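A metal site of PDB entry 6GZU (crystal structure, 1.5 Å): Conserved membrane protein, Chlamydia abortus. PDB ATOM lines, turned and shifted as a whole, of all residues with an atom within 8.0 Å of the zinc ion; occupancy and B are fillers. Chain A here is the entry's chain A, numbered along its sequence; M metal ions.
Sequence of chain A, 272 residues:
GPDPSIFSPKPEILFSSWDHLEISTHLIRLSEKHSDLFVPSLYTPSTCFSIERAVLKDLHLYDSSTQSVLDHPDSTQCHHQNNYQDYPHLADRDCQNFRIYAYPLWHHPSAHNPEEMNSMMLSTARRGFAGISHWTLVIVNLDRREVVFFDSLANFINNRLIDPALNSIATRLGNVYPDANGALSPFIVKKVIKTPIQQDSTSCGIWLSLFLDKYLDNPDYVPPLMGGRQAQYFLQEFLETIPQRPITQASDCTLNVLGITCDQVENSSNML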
ATOM      1  N   PHE A  38     -16.456 -21.420  -8.882  1.00  0.00           N
ATOM      2  CA  PHE A  38     -15.129 -21.807  -9.288  1.00  0.00           C
ATOM      3  C   PHE A  38     -14.321 -20.568  -9.705  1.00  0.00           C
ATOM      4  O   PHE A  38     -14.726 -19.786 -10.588  1.00  0.00           O
ATOM      5  CB  PHE A  38     -15.217 -22.757 -10.468  1.00  0.00           C
ATOM      6  CG  PHE A  38     -13.907 -23.169 -11.032  1.00  0.00           C
ATOM      7  CD1 PHE A  38     -13.311 -22.432 -12.064  1.00  0.00           C
ATOM      8  CD2 PHE A  38     -13.282 -24.326 -10.608  1.00  0.00           C
ATOM      9  CE1 PHE A  38     -12.113 -22.814 -12.603  1.00  0.00           C
ATOM     10  CE2 PHE A  38     -12.055 -24.719 -11.168  1.00  0.00           C
ATOM     11  CZ  PHE A  38     -11.471 -23.964 -12.140  1.00  0.00           C
ATOM     12  N   LYS A  57     -11.170 -27.264 -20.140  1.00  0.00           N
ATOM     13  CA  LYS A  57     -10.254 -27.964 -19.202  1.00  0.00           C
ATOM     14  C   LYS A  57     -10.814 -27.902 -17.786  1.00  0.00           C
ATOM     15  O   LYS A  57     -10.764 -28.895 -17.045  1.00  0.00           O
ATOM     16  CB  LYS A  57      -8.838 -27.382 -19.227  1.00  0.00           C
ATOM     17  CG  LYS A  57      -8.034 -27.763 -20.494  1.00  0.00           C
ATOM     18  CD  LYS A  57      -6.692 -27.003 -20.553  1.00  0.00           C
ATOM     19  CE  LYS A  57      -5.793 -27.402 -19.385  1.00  0.00           C
ATOM     20  NZ  LYS A  57      -5.556 -28.891 -19.319  1.00  0.00           N
ATOM     21  N   ASP A  58     -11.384 -26.771 -17.375  1.00  0.00           N
ATOM     22  CA  ASP A  58     -11.870 -26.688 -15.977  1.00  0.00           C
ATOM     23  C   ASP A  58     -13.089 -27.570 -15.722  1.00  0.00           C
ATOM     24  O   ASP A  58     -13.300 -28.016 -14.598  1.00  0.00           O
ATOM     25  CB  ASP A  58     -12.170 -25.221 -15.602  1.00  0.00           C
ATOM     26  CG  ASP A  58     -10.929 -24.416 -15.417  1.00  0.00           C
ATOM     27  OD1 ASP A  58      -9.911 -25.016 -15.022  1.00  0.00           O
ATOM     28  OD2 ASP A  58     -10.943 -23.205 -15.620  1.00  0.00           O
ATOM     29  N   LEU A  59     -13.842 -27.893 -16.782  1.00  0.00           N
ATOM     30  CA  LEU A  59     -14.969 -28.834 -16.667  1.00  0.00           C
ATOM     31  C   LEU A  59     -14.549 -30.266 -17.004  1.00  0.00           C
ATOM     32  O   LEU A  59     -15.422 -31.150 -17.147  1.00  0.00           O
ATOM     33  CB  LEU A  59     -16.091 -28.411 -17.621  1.00  0.00           C
ATOM     34  CG  LEU A  59     -16.668 -27.053 -17.184  1.00  0.00           C
ATOM     35  CD1 LEU A  59     -17.613 -26.507 -18.305  1.00  0.00           C
ATOM     36  CD2 LEU A  59     -17.402 -27.274 -15.916  1.00  0.00           C
ATOM     37  N   HIS A  60     -13.244 -30.504 -17.103  1.00  0.00           N
ATOM     38  CA  HIS A  60     -12.699 -31.837 -17.440  1.00  0.00           C
ATOM     39  C   HIS A  60     -13.214 -32.417 -18.751  1.00  0.00           C
ATOM     40  O   HIS A  60     -13.393 -33.647 -18.865  1.00  0.00           O
ATOM     41  CB  HIS A  60     -12.895 -32.804 -16.260  1.00  0.00           C
ATOM     42  CG  HIS A  60     -12.481 -32.195 -14.955  1.00  0.00           C
ATOM     43  ND1 HIS A  60     -13.378 -31.630 -14.065  1.00  0.00           N
ATOM     44  CD2 HIS A  60     -11.255 -31.992 -14.431  1.00  0.00           C
ATOM     45  CE1 HIS A  60     -12.726 -31.169 -13.013  1.00  0.00           C
ATOM     46  NE2 HIS A  60     -11.435 -31.375 -13.194  1.00  0.00           N
ATOM     47  N   ASP A  74     -14.159 -36.200 -17.793  1.00  0.00           N
ATOM     48  CA  ASP A  74     -13.248 -37.287 -17.487  1.00  0.00           C
ATOM     49  C   ASP A  74     -12.329 -36.767 -16.390  1.00  0.00           C
ATOM     50  O   ASP A  74     -11.435 -35.960 -16.644  1.00  0.00           O
ATOM     51  CB  ASP A  74     -12.457 -37.669 -18.733  1.00  0.00           C
ATOM     52  CG  ASP A  74     -11.432 -38.729 -18.469  1.00  0.00           C
ATOM     53  OD1 ASP A  74     -11.358 -39.251 -17.327  1.00  0.00           O
ATOM     54  OD2 ASP A  74     -10.698 -39.088 -19.430  1.00  0.00           O
ATOM     55  N   SER A  75     -12.574 -37.210 -15.164  1.00  0.00           N
ATOM     56  CA  SER A  75     -11.901 -36.626 -14.006  1.00  0.00           C
ATOM     57  C   SER A  75     -10.411 -36.966 -13.975  1.00  0.00           C
ATOM     58  O   SER A  75      -9.647 -36.320 -13.265  1.00  0.00           O
ATOM     59  CB  SER A  75     -12.562 -37.099 -12.726  1.00  0.00           C
ATOM     60  OG  SER A  75     -12.508 -38.503 -12.656  1.00  0.00           O
ATOM     61  N   THR A  76     -10.003 -37.964 -14.753  1.00  0.00           N
ATOM     62  CA  THR A  76      -8.596 -38.283 -14.930  1.00  0.00           C
ATOM     63  C   THR A  76      -7.859 -37.207 -15.757  1.00  0.00           C
ATOM     64  O   THR A  76      -6.627 -37.193 -15.788  1.00  0.00           O
ATOM     65  CB  THR A  76      -8.419 -39.683 -15.556  1.00  0.00           C
ATOM     66  OG1 THR A  76      -8.715 -39.660 -16.959  1.00  0.00           O
ATOM     67  CG2 THR A  76      -9.361 -40.635 -14.879  1.00  0.00           C
ATOM     68  N   GLN A  77      -8.586 -36.295 -16.400  1.00  0.00           N
ATOM     69  CA  GLN A  77      -7.923 -35.202 -17.113  1.00  0.00           C
ATOM     70  C   GLN A  77      -7.689 -33.997 -16.243  1.00  0.00           C
ATOM     71  O   GLN A  77      -7.205 -32.977 -16.713  1.00  0.00           O
ATOM     72  CB  GLN A  77      -8.737 -34.784 -18.341  1.00  0.00           C
ATOM     73  CG  GLN A  77      -9.167 -35.960 -19.169  1.00  0.00           C
ATOM     74  CD  GLN A  77      -8.028 -36.594 -19.938  1.00  0.00           C
ATOM     75  OE1 GLN A  77      -6.944 -36.026 -20.069  1.00  0.00           O
ATOM     76  NE2 GLN A  77      -8.279 -37.771 -20.476  1.00  0.00           N
ATOM     77  N   CYS A  78      -8.048 -34.104 -14.975  1.00  0.00           N
ATOM     78  CA  CYS A  78      -8.025 -32.963 -14.084  1.00  0.00           C
ATOM     79  C   CYS A  78      -6.638 -32.371 -13.866  1.00  0.00           C
ATOM     80  O   CYS A  78      -5.727 -33.061 -13.422  1.00  0.00           O
ATOM     81  CB  CYS A  78      -8.588 -33.396 -12.755  1.00  0.00           C
ATOM     82  SG  CYS A  78      -8.404 -32.176 -11.530  1.00  0.00           S
ATOM     83  N   HIS A  79      -6.493 -31.066 -14.110  1.00  0.00           N
ATOM     84  CA  HIS A  79      -5.218 -30.371 -13.865  1.00  0.00           C
ATOM     85  C   HIS A  79      -5.291 -29.448 -12.610  1.00  0.00           C
ATOM     86  O   HIS A  79      -4.392 -28.598 -12.345  1.00  0.00           O
ATOM     87  CB  HIS A  79      -4.819 -29.588 -15.120  1.00  0.00           C
ATOM     88  CG  HIS A  79      -5.690 -28.404 -15.409  1.00  0.00           C
ATOM     89  ND1 HIS A  79      -7.062 -28.448 -15.315  1.00  0.00           N
ATOM     90  CD2 HIS A  79      -5.383 -27.143 -15.791  1.00  0.00           C
ATOM     91  CE1 HIS A  79      -7.566 -27.252 -15.601  1.00  0.00           C
ATOM     92  NE2 HIS A  79      -6.567 -26.450 -15.913  1.00  0.00           N
ATOM     93  N   HIS A  80      -6.346 -29.628 -11.818  1.00  0.00           N
ATOM     94  CA  HIS A  80      -6.560 -28.792 -10.633  1.00  0.00           C
ATOM     95  C   HIS A  80      -5.923 -29.241  -9.349  1.00  0.00           C
ATOM     96  O   HIS A  80      -5.883 -28.474  -8.387  1.00  0.00           O
ATOM     97  CB  HIS A  80      -8.040 -28.635 -10.332  1.00  0.00           C
ATOM     98  CG  HIS A  80      -8.827 -28.141 -11.499  1.00  0.00           C
ATOM     99  ND1 HIS A  80      -9.759 -28.932 -12.142  1.00  0.00           N
ATOM    100  CD2 HIS A  80      -8.806 -26.949 -12.136  1.00  0.00           C
ATOM    101  CE1 HIS A  80     -10.291 -28.215 -13.130  1.00  0.00           C
ATOM    102  NE2 HIS A  80      -9.706 -27.023 -13.162  1.00  0.00           N
ATOM    103  N   GLN A  81      -5.451 -30.466  -9.309  1.00  0.00           N
ATOM    104  CA  GLN A  81      -4.875 -30.955  -8.077  1.00  0.00           C
ATOM    105  C   GLN A  81      -3.353 -30.776  -8.065  1.00  0.00           C
ATOM    106  O   GLN A  81      -2.689 -30.859  -9.103  1.00  0.00           O
ATOM    107  CB  GLN A  81      -5.347 -32.393  -7.824  1.00  0.00           C
ATOM    108  CG  GLN A  81      -6.869 -32.463  -7.596  1.00  0.00           C
ATOM    109  N   TYR A  87      -3.705 -23.047  -9.161  1.00  0.00           N
ATOM    110  CA  TYR A  87      -4.856 -23.426  -8.341  1.00  0.00           C
ATOM    111  C   TYR A  87      -4.531 -23.750  -6.886  1.00  0.00           C
ATOM    112  O   TYR A  87      -4.960 -24.778  -6.389  1.00  0.00           O
ATOM    113  CB  TYR A  87      -5.621 -24.636  -8.949  1.00  0.00           C
ATOM    114  CG  TYR A  87      -5.936 -24.442 -10.420  1.00  0.00           C
ATOM    115  CD1 TYR A  87      -6.905 -23.551 -10.831  1.00  0.00           C
ATOM    116  CD2 TYR A  87      -5.257 -25.192 -11.406  1.00  0.00           C
ATOM    117  CE1 TYR A  87      -7.191 -23.369 -12.182  1.00  0.00           C
ATOM    118  CE2 TYR A  87      -5.531 -25.009 -12.778  1.00  0.00           C
ATOM    119  CZ  TYR A  87      -6.499 -24.099 -13.140  1.00  0.00           C
ATOM    120  OH  TYR A  87      -6.742 -23.905 -14.465  1.00  0.00           O
ATOM    121  N   LEU A  90      -7.599 -24.543  -4.852  1.00  0.00           N
ATOM    122  CA  LEU A  90      -8.348 -25.782  -5.116  1.00  0.00           C
ATOM    123  C   LEU A  90      -7.685 -27.009  -4.515  1.00  0.00           C
ATOM    124  O   LEU A  90      -8.233 -28.109  -4.586  1.00  0.00           O
ATOM    125  CB  LEU A  90      -8.521 -26.026  -6.620  1.00  0.00           C
ATOM    126  CG  LEU A  90      -9.314 -24.925  -7.339  1.00  0.00           C
ATOM    127  CD1 LEU A  90      -9.494 -25.234  -8.825  1.00  0.00           C
ATOM    128  CD2 LEU A  90     -10.664 -24.680  -6.623  1.00  0.00           C
ATOM    129  N   ARG A  93     -10.221 -28.484  -2.273  1.00  0.00           N
ATOM    130  CA  ARG A  93     -11.608 -28.551  -2.760  1.00  0.00           C
ATOM    131  C   ARG A  93     -11.820 -29.722  -3.716  1.00  0.00           C
ATOM    132  O   ARG A  93     -10.893 -30.188  -4.387  1.00  0.00           O
ATOM    133  CB  ARG A  93     -12.027 -27.317  -3.602  1.00  0.00           C
ATOM    134  CG  ARG A  93     -11.645 -25.925  -3.137  1.00  0.00           C
ATOM    135  CD  ARG A  93     -12.456 -25.446  -1.971  1.00  0.00           C
ATOM    136  NE  ARG A  93     -13.911 -25.453  -2.147  1.00  0.00           N
ATOM    137  CZ  ARG A  93     -14.637 -24.411  -2.572  1.00  0.00           C
ATOM    138  NH1 ARG A  93     -14.052 -23.275  -2.961  1.00  0.00           N
ATOM    139  NH2 ARG A  93     -15.948 -24.508  -2.628  1.00  0.00           N
ATOM    140  N   ASP A  94     -13.067 -30.140  -3.852  1.00  0.00           N
ATOM    141  CA  ASP A  94     -13.423 -31.021  -4.950  1.00  0.00           C
ATOM    142  C   ASP A  94     -13.713 -30.192  -6.200  1.00  0.00           C
ATOM    143  O   ASP A  94     -14.776 -29.552  -6.304  1.00  0.00           O
ATOM    144  CB  ASP A  94     -14.651 -31.844  -4.589  1.00  0.00           C
ATOM    145  CG  ASP A  94     -15.170 -32.629  -5.756  1.00  0.00           C
ATOM    146  OD1 ASP A  94     -14.425 -32.808  -6.759  1.00  0.00           O
ATOM    147  OD2 ASP A  94     -16.321 -33.099  -5.672  1.00  0.00           O
ATOM    148  N   CYS A  95     -12.774 -30.261  -7.148  1.00  0.00           N
ATOM    149  CA  CYS A  95     -12.766 -29.361  -8.307  1.00  0.00           C
ATOM    150  C   CYS A  95     -13.938 -29.610  -9.213  1.00  0.00           C
ATOM    151  O   CYS A  95     -14.212 -28.810 -10.118  1.00  0.00           O
ATOM    152  CB  CYS A  95     -11.457 -29.503  -9.082  1.00  0.00           C
ATOM    153  SG  CYS A  95     -11.190 -31.112  -9.731  1.00  0.00           S
ATOM    154  N   GLN A  96     -14.637 -30.720  -8.980  1.00  0.00           N
ATOM    155  CA  GLN A  96     -15.849 -31.030  -9.746  1.00  0.00           C
ATOM    156  C   GLN A  96     -17.099 -30.328  -9.238  1.00  0.00           C
ATOM    157  O   GLN A  96     -18.004 -30.046 -10.021  1.00  0.00           O
ATOM    158  CB  GLN A  96     -16.085 -32.546  -9.764  1.00  0.00           C
ATOM    159  CG  GLN A  96     -15.021 -33.330 -10.501  1.00  0.00           C
ATOM    160  CD  GLN A  96     -14.719 -34.686  -9.850  1.00  0.00           C
ATOM    161  OE1 GLN A  96     -13.555 -35.083  -9.709  1.00  0.00           O
ATOM    162  NE2 GLN A  96     -15.768 -35.401  -9.433  1.00  0.00           N
ATOM    163  N   ASN A  97     -17.137 -30.003  -7.950  1.00  0.00           N
ATOM    164  CA  ASN A  97     -18.362 -29.626  -7.247  1.00  0.00           C
ATOM    165  C   ASN A  97     -18.858 -28.164  -7.422  1.00  0.00           C
ATOM    166  O   ASN A  97     -19.544 -27.587  -6.569  1.00  0.00           O
ATOM    167  CB  ASN A  97     -18.157 -29.913  -5.758  1.00  0.00           C
ATOM    168  CG  ASN A  97     -19.462 -30.035  -5.025  1.00  0.00           C
ATOM    169  OD1 ASN A  97     -20.499 -30.280  -5.639  1.00  0.00           O
ATOM    170  ND2 ASN A  97     -19.426 -29.873  -3.694  1.00  0.00           N
ATOM    171  N   PHE A  98     -18.529 -27.541  -8.533  1.00  0.00           N
ATOM    172  CA  PHE A  98     -18.888 -26.144  -8.701  1.00  0.00           C
ATOM    173  C   PHE A  98     -20.020 -25.953  -9.709  1.00  0.00           C
ATOM    174  O   PHE A  98     -20.230 -26.833 -10.576  1.00  0.00           O
ATOM    175  CB  PHE A  98     -17.652 -25.365  -9.159  1.00  0.00           C
ATOM    176  CG  PHE A  98     -16.566 -25.355  -8.139  1.00  0.00           C
ATOM    177  CD1 PHE A  98     -16.650 -24.467  -7.080  1.00  0.00           C
ATOM    178  CD2 PHE A  98     -15.462 -26.187  -8.248  1.00  0.00           C
ATOM    179  CE1 PHE A  98     -15.663 -24.424  -6.118  1.00  0.00           C
ATOM    180  CE2 PHE A  98     -14.465 -26.148  -7.266  1.00  0.00           C
ATOM    181  CZ  PHE A  98     -14.564 -25.228  -6.220  1.00  0.00           C
ATOM    182  N   TYR A 101     -18.757 -20.587 -13.023  1.00  0.00           N
ATOM    183  CA  TYR A 101     -17.341 -20.476 -13.359  1.00  0.00           C
ATOM    184  C   TYR A 101     -17.120 -19.092 -13.931  1.00  0.00           C
ATOM    185  O   TYR A 101     -17.681 -18.763 -14.965  1.00  0.00           O
ATOM    186  CB  TYR A 101     -16.975 -21.537 -14.409  1.00  0.00           C
ATOM    187  CG  TYR A 101     -17.017 -22.960 -13.866  1.00  0.00           C
ATOM    188  CD1 TYR A 101     -18.225 -23.552 -13.492  1.00  0.00           C
ATOM    189  CD2 TYR A 101     -15.848 -23.747 -13.794  1.00  0.00           C
ATOM    190  CE1 TYR A 101     -18.242 -24.864 -12.983  1.00  0.00           C
ATOM    191  CE2 TYR A 101     -15.862 -25.055 -13.326  1.00  0.00           C
ATOM    192  CZ  TYR A 101     -17.061 -25.598 -12.908  1.00  0.00           C
ATOM    193  OH  TYR A 101     -17.103 -26.893 -12.399  1.00  0.00           O
HETATM  194 ZN    ZN M   1     -10.229 -30.875 -11.713  1.00  0.00          ZN
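OD1 of Asp 58 is in hydrogen-bond range of NE2 of His 80. The backbone carbonyl oxygen (O) of His 60 is in hydrogen-bond range of the backbone NH (N) of Asp 74 (2.9 Å).
Of the 22 residues printed, 4 come within 4 Å of the zinc ion. The nearest printed residue that does not touch the zinc ion is His 79 (4.4 Å).
NE2 of His 60 binds the zinc ion. ND1 of His 80 binds the zinc ion, at 2.0 Å. The zinc ion is bound by SG of Cys 95 (2.2 Å). SG of Cys 78 binds the zinc ion (2.2 Å).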
